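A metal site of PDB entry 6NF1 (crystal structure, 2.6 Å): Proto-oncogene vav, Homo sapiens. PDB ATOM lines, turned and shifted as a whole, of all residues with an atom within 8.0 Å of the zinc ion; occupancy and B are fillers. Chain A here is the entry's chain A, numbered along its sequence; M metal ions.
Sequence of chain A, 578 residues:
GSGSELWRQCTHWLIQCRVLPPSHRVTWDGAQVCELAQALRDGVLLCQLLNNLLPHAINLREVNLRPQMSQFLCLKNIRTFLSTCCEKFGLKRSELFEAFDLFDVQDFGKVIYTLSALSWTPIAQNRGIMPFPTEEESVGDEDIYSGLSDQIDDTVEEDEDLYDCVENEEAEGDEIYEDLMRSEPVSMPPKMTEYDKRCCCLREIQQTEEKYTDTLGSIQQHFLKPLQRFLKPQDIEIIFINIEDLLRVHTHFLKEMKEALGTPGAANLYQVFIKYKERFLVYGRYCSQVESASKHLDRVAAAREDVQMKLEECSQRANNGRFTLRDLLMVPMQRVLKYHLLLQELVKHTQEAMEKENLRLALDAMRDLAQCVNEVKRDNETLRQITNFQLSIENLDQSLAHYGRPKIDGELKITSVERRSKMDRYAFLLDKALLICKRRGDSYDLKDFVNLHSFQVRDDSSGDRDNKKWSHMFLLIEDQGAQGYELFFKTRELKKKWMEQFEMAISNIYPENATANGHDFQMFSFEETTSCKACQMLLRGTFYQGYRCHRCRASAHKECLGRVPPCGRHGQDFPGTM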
ATOM      1  N   ALA A 514      -4.029 -19.654 -29.770  1.00  0.00           N
ATOM      2  CA  ALA A 514      -5.152 -20.078 -30.605  1.00  0.00           C
ATOM      3  C   ALA A 514      -5.010 -21.510 -31.090  1.00  0.00           C
ATOM      4  O   ALA A 514      -6.017 -22.234 -31.224  1.00  0.00           O
ATOM      5  CB  ALA A 514      -5.278 -19.162 -31.803  1.00  0.00           C
ATOM      6  N   ALA A 516      -2.734 -23.726 -29.595  1.00  0.00           N
ATOM      7  CA  ALA A 516      -2.182 -24.503 -28.481  1.00  0.00           C
ATOM      8  C   ALA A 516      -3.072 -25.710 -28.142  1.00  0.00           C
ATOM      9  O   ALA A 516      -4.297 -25.648 -28.337  1.00  0.00           O
ATOM     10  CB  ALA A 516      -1.987 -23.615 -27.259  1.00  0.00           C
ATOM     11  N   ASN A 517      -2.417 -26.814 -27.696  1.00  0.00           N
ATOM     12  CA  ASN A 517      -2.969 -28.097 -27.240  1.00  0.00           C
ATOM     13  C   ASN A 517      -4.047 -28.726 -28.148  1.00  0.00           C
ATOM     14  O   ASN A 517      -5.108 -29.146 -27.668  1.00  0.00           O
ATOM     15  CB  ASN A 517      -3.475 -27.980 -25.800  1.00  0.00           C
ATOM     16  CG  ASN A 517      -2.416 -27.508 -24.824  1.00  0.00           C
ATOM     17  OD1 ASN A 517      -2.547 -26.458 -24.195  1.00  0.00           O
ATOM     18  ND2 ASN A 517      -1.313 -28.263 -24.710  1.00  0.00           N
ATOM     19  N   GLY A 518      -3.735 -28.816 -29.447  1.00  0.00           N
ATOM     20  CA  GLY A 518      -4.607 -29.416 -30.461  1.00  0.00           C
ATOM     21  C   GLY A 518      -5.775 -28.573 -30.931  1.00  0.00           C
ATOM     22  O   GLY A 518      -6.453 -28.946 -31.893  1.00  0.00           O
ATOM     23  N   HIS A 519      -6.028 -27.433 -30.261  1.00  0.00           N
ATOM     24  CA  HIS A 519      -7.142 -26.531 -30.567  1.00  0.00           C
ATOM     25  C   HIS A 519      -6.932 -25.742 -31.859  1.00  0.00           C
ATOM     26  O   HIS A 519      -5.799 -25.446 -32.245  1.00  0.00           O
ATOM     27  CB  HIS A 519      -7.386 -25.520 -29.418  1.00  0.00           C
ATOM     28  CG  HIS A 519      -7.691 -26.123 -28.076  1.00  0.00           C
ATOM     29  ND1 HIS A 519      -8.870 -26.780 -27.848  1.00  0.00           N
ATOM     30  CD2 HIS A 519      -7.002 -26.030 -26.919  1.00  0.00           C
ATOM     31  CE1 HIS A 519      -8.838 -27.130 -26.574  1.00  0.00           C
ATOM     32  NE2 HIS A 519      -7.737 -26.689 -25.977  1.00  0.00           N
ATOM     33  N   ASP A 520      -8.044 -25.339 -32.475  1.00  0.00           N
ATOM     34  CA  ASP A 520      -8.075 -24.446 -33.643  1.00  0.00           C
ATOM     35  C   ASP A 520      -9.089 -23.328 -33.265  1.00  0.00           C
ATOM     36  O   ASP A 520     -10.260 -23.346 -33.706  1.00  0.00           O
ATOM     37  CB  ASP A 520      -8.468 -25.217 -34.924  1.00  0.00           C
ATOM     38  CG  ASP A 520      -8.449 -24.403 -36.206  1.00  0.00           C
ATOM     39  OD1 ASP A 520      -7.851 -23.304 -36.210  1.00  0.00           O
ATOM     40  OD2 ASP A 520      -9.009 -24.875 -37.210  1.00  0.00           O
ATOM     41  N   PHE A 521      -8.655 -22.400 -32.361  1.00  0.00           N
ATOM     42  CA  PHE A 521      -9.478 -21.282 -31.877  1.00  0.00           C
ATOM     43  C   PHE A 521      -9.595 -20.191 -32.896  1.00  0.00           C
ATOM     44  O   PHE A 521      -8.586 -19.652 -33.359  1.00  0.00           O
ATOM     45  CB  PHE A 521      -9.000 -20.724 -30.531  1.00  0.00           C
ATOM     46  CG  PHE A 521      -9.494 -21.475 -29.329  1.00  0.00           C
ATOM     47  CD1 PHE A 521     -10.843 -21.433 -28.964  1.00  0.00           C
ATOM     48  CD2 PHE A 521      -8.618 -22.185 -28.517  1.00  0.00           C
ATOM     49  CE1 PHE A 521     -11.304 -22.130 -27.842  1.00  0.00           C
ATOM     50  CE2 PHE A 521      -9.076 -22.872 -27.394  1.00  0.00           C
ATOM     51  CZ  PHE A 521     -10.427 -22.856 -27.068  1.00  0.00           C
ATOM     52  N   ARG A 548     -13.806 -19.789 -30.414  1.00  0.00           N
ATOM     53  CA  ARG A 548     -14.341 -21.144 -30.418  1.00  0.00           C
ATOM     54  C   ARG A 548     -13.413 -22.099 -31.156  1.00  0.00           C
ATOM     55  O   ARG A 548     -12.832 -21.725 -32.170  1.00  0.00           O
ATOM     56  CB  ARG A 548     -15.758 -21.209 -31.006  1.00  0.00           C
ATOM     57  CG  ARG A 548     -16.556 -22.442 -30.615  1.00  0.00           C
ATOM     58  CD  ARG A 548     -17.916 -22.452 -31.280  1.00  0.00           C
ATOM     59  NE  ARG A 548     -18.470 -23.815 -31.324  1.00  0.00           N
ATOM     60  CZ  ARG A 548     -18.465 -24.593 -32.400  1.00  0.00           C
ATOM     61  NH1 ARG A 548     -17.965 -24.160 -33.556  1.00  0.00           N
ATOM     62  NH2 ARG A 548     -18.973 -25.817 -32.340  1.00  0.00           N
ATOM     63  N   CYS A 549     -13.262 -23.310 -30.626  1.00  0.00           N
ATOM     64  CA  CYS A 549     -12.481 -24.346 -31.290  1.00  0.00           C
ATOM     65  C   CYS A 549     -13.489 -25.239 -31.983  1.00  0.00           C
ATOM     66  O   CYS A 549     -14.331 -25.829 -31.314  1.00  0.00           O
ATOM     67  CB  CYS A 549     -11.619 -25.122 -30.310  1.00  0.00           C
ATOM     68  SG  CYS A 549     -10.918 -26.638 -30.995  1.00  0.00           S
ATOM     69  N   HIS A 550     -13.434 -25.321 -33.334  1.00  0.00           N
ATOM     70  CA  HIS A 550     -14.369 -26.157 -34.096  1.00  0.00           C
ATOM     71  C   HIS A 550     -14.216 -27.643 -33.766  1.00  0.00           C
ATOM     72  O   HIS A 550     -15.182 -28.405 -33.848  1.00  0.00           O
ATOM     73  CB  HIS A 550     -14.256 -25.894 -35.611  1.00  0.00           C
ATOM     74  CG  HIS A 550     -13.068 -26.534 -36.268  1.00  0.00           C
ATOM     75  ND1 HIS A 550     -13.181 -27.735 -36.946  1.00  0.00           N
ATOM     76  CD2 HIS A 550     -11.793 -26.098 -36.341  1.00  0.00           C
ATOM     77  CE1 HIS A 550     -11.962 -28.003 -37.405  1.00  0.00           C
ATOM     78  NE2 HIS A 550     -11.095 -27.045 -37.063  1.00  0.00           N
ATOM     79  N   ARG A 551     -13.005 -28.035 -33.339  1.00  0.00           N
ATOM     80  CA  ARG A 551     -12.668 -29.404 -32.996  1.00  0.00           C
ATOM     81  C   ARG A 551     -13.351 -29.910 -31.721  1.00  0.00           C
ATOM     82  O   ARG A 551     -14.053 -30.918 -31.800  1.00  0.00           O
ATOM     83  CB  ARG A 551     -11.132 -29.586 -32.938  1.00  0.00           C
ATOM     84  CG  ARG A 551     -10.462 -29.286 -34.259  1.00  0.00           C
ATOM     85  CD  ARG A 551      -8.949 -29.263 -34.188  1.00  0.00           C
ATOM     86  NE  ARG A 551      -8.398 -29.032 -35.516  1.00  0.00           N
ATOM     87  CZ  ARG A 551      -7.112 -28.842 -35.795  1.00  0.00           C
ATOM     88  NH1 ARG A 551      -6.210 -28.843 -34.815  1.00  0.00           N
ATOM     89  NH2 ARG A 551      -6.718 -28.634 -37.041  1.00  0.00           N
ATOM     90  N   CYS A 552     -13.202 -29.221 -30.576  1.00  0.00           N
ATOM     91  CA  CYS A 552     -13.825 -29.674 -29.313  1.00  0.00           C
ATOM     92  C   CYS A 552     -15.004 -28.823 -28.824  1.00  0.00           C
ATOM     93  O   CYS A 552     -15.513 -29.068 -27.718  1.00  0.00           O
ATOM     94  CB  CYS A 552     -12.770 -29.814 -28.224  1.00  0.00           C
ATOM     95  SG  CYS A 552     -11.947 -28.270 -27.783  1.00  0.00           S
ATOM     96  N   ARG A 553     -15.440 -27.819 -29.625  1.00  0.00           N
ATOM     97  CA  ARG A 553     -16.545 -26.908 -29.291  1.00  0.00           C
ATOM     98  C   ARG A 553     -16.293 -26.081 -27.985  1.00  0.00           C
ATOM     99  O   ARG A 553     -17.242 -25.666 -27.324  1.00  0.00           O
ATOM    100  CB  ARG A 553     -17.906 -27.650 -29.272  1.00  0.00           C
ATOM    101  N   ALA A 554     -15.002 -25.857 -27.627  1.00  0.00           N
ATOM    102  CA  ALA A 554     -14.643 -25.065 -26.448  1.00  0.00           C
ATOM    103  C   ALA A 554     -14.720 -23.577 -26.788  1.00  0.00           C
ATOM    104  O   ALA A 554     -14.317 -23.168 -27.880  1.00  0.00           O
ATOM    105  CB  ALA A 554     -13.233 -25.408 -25.967  1.00  0.00           C
ATOM    106  N   SER A 555     -15.273 -22.771 -25.858  1.00  0.00           N
ATOM    107  CA  SER A 555     -15.459 -21.343 -26.021  1.00  0.00           C
ATOM    108  C   SER A 555     -14.656 -20.599 -24.966  1.00  0.00           C
ATOM    109  O   SER A 555     -14.735 -20.942 -23.776  1.00  0.00           O
ATOM    110  CB  SER A 555     -16.927 -20.978 -25.959  1.00  0.00           C
ATOM    111  OG  SER A 555     -17.519 -21.193 -24.690  1.00  0.00           O
ATOM    112  N   VAL A 564      -6.972 -23.119 -21.229  1.00  0.00           N
ATOM    113  CA  VAL A 564      -8.013 -24.061 -21.677  1.00  0.00           C
ATOM    114  C   VAL A 564      -7.463 -25.512 -21.779  1.00  0.00           C
ATOM    115  O   VAL A 564      -6.492 -25.728 -22.507  1.00  0.00           O
ATOM    116  CB  VAL A 564      -8.699 -23.590 -22.994  1.00  0.00           C
ATOM    117  CG1 VAL A 564      -9.789 -24.566 -23.449  1.00  0.00           C
ATOM    118  CG2 VAL A 564      -9.269 -22.189 -22.869  1.00  0.00           C
ATOM    119  N   PRO A 565      -8.110 -26.504 -21.112  1.00  0.00           N
ATOM    120  CA  PRO A 565      -7.668 -27.916 -21.235  1.00  0.00           C
ATOM    121  C   PRO A 565      -7.536 -28.432 -22.683  1.00  0.00           C
ATOM    122  O   PRO A 565      -8.232 -27.909 -23.559  1.00  0.00           O
ATOM    123  CB  PRO A 565      -8.744 -28.697 -20.467  1.00  0.00           C
ATOM    124  CG  PRO A 565      -9.899 -27.743 -20.323  1.00  0.00           C
ATOM    125  CD  PRO A 565      -9.278 -26.399 -20.207  1.00  0.00           C
ATOM    126  N   PRO A 566      -6.670 -29.438 -22.962  1.00  0.00           N
ATOM    127  CA  PRO A 566      -6.438 -29.862 -24.358  1.00  0.00           C
ATOM    128  C   PRO A 566      -7.612 -30.403 -25.158  1.00  0.00           C
ATOM    129  O   PRO A 566      -8.632 -30.806 -24.620  1.00  0.00           O
ATOM    130  CB  PRO A 566      -5.359 -30.951 -24.227  1.00  0.00           C
ATOM    131  CG  PRO A 566      -4.681 -30.655 -22.941  1.00  0.00           C
ATOM    132  CD  PRO A 566      -5.751 -30.131 -22.029  1.00  0.00           C
ATOM    133  N   CYS A 567      -7.422 -30.412 -26.494  1.00  0.00           N
ATOM    134  CA  CYS A 567      -8.347 -30.901 -27.515  1.00  0.00           C
ATOM    135  C   CYS A 567      -8.142 -32.439 -27.660  1.00  0.00           C
ATOM    136  O   CYS A 567      -7.092 -32.974 -27.281  1.00  0.00           O
ATOM    137  CB  CYS A 567      -8.060 -30.164 -28.823  1.00  0.00           C
ATOM    138  SG  CYS A 567      -9.475 -30.021 -29.935  1.00  0.00           S
ATOM    139  N   GLY A 568      -9.157 -33.120 -28.223  1.00  0.00           N
ATOM    140  CA  GLY A 568      -9.148 -34.564 -28.434  1.00  0.00           C
ATOM    141  C   GLY A 568      -9.061 -34.983 -29.883  1.00  0.00           C
ATOM    142  O   GLY A 568      -8.645 -36.100 -30.194  1.00  0.00           O
HETATM  143 ZN    ZN M   1     -10.149 -27.686 -28.952  1.00  0.00          ZN
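NE2 of His 519 lies within hydrogen-bond range of O of Pro 565 (2.8 Å).
N of Arg 551 lies close to SG of Cys 549, 3.4 Å away.
SG of Cys 549 lies close to N of Asp 520.
N of Cys 549 is in hydrogen-bond range of O of Ala 554 (2.9 Å).
The side-chain sulfur of Cys 567 sits close to the backbone carbonyl oxygen of Gly 518, at 3.8 Å.
N of Cys 567 lies within hydrogen-bond range of O of Asn 517 (2.9 Å).
Four residues have an atom within 4 Å of the zinc ion: His 519, Cys 549, Cys 552 and Cys 567.
The nearest printed residue that does not touch the zinc ion is Arg 551 (4.5 Å).
The zinc ion is bound by a ring nitrogen (ND1) of His 519 (1.9 Å), the side-chain sulfur (SG) of Cys 552 (2.2 Å), the side-chain sulfur (SG) of Cys 549 (2.4 Å) and the side-chain sulfur (SG) of Cys 567 (2.6 Å).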
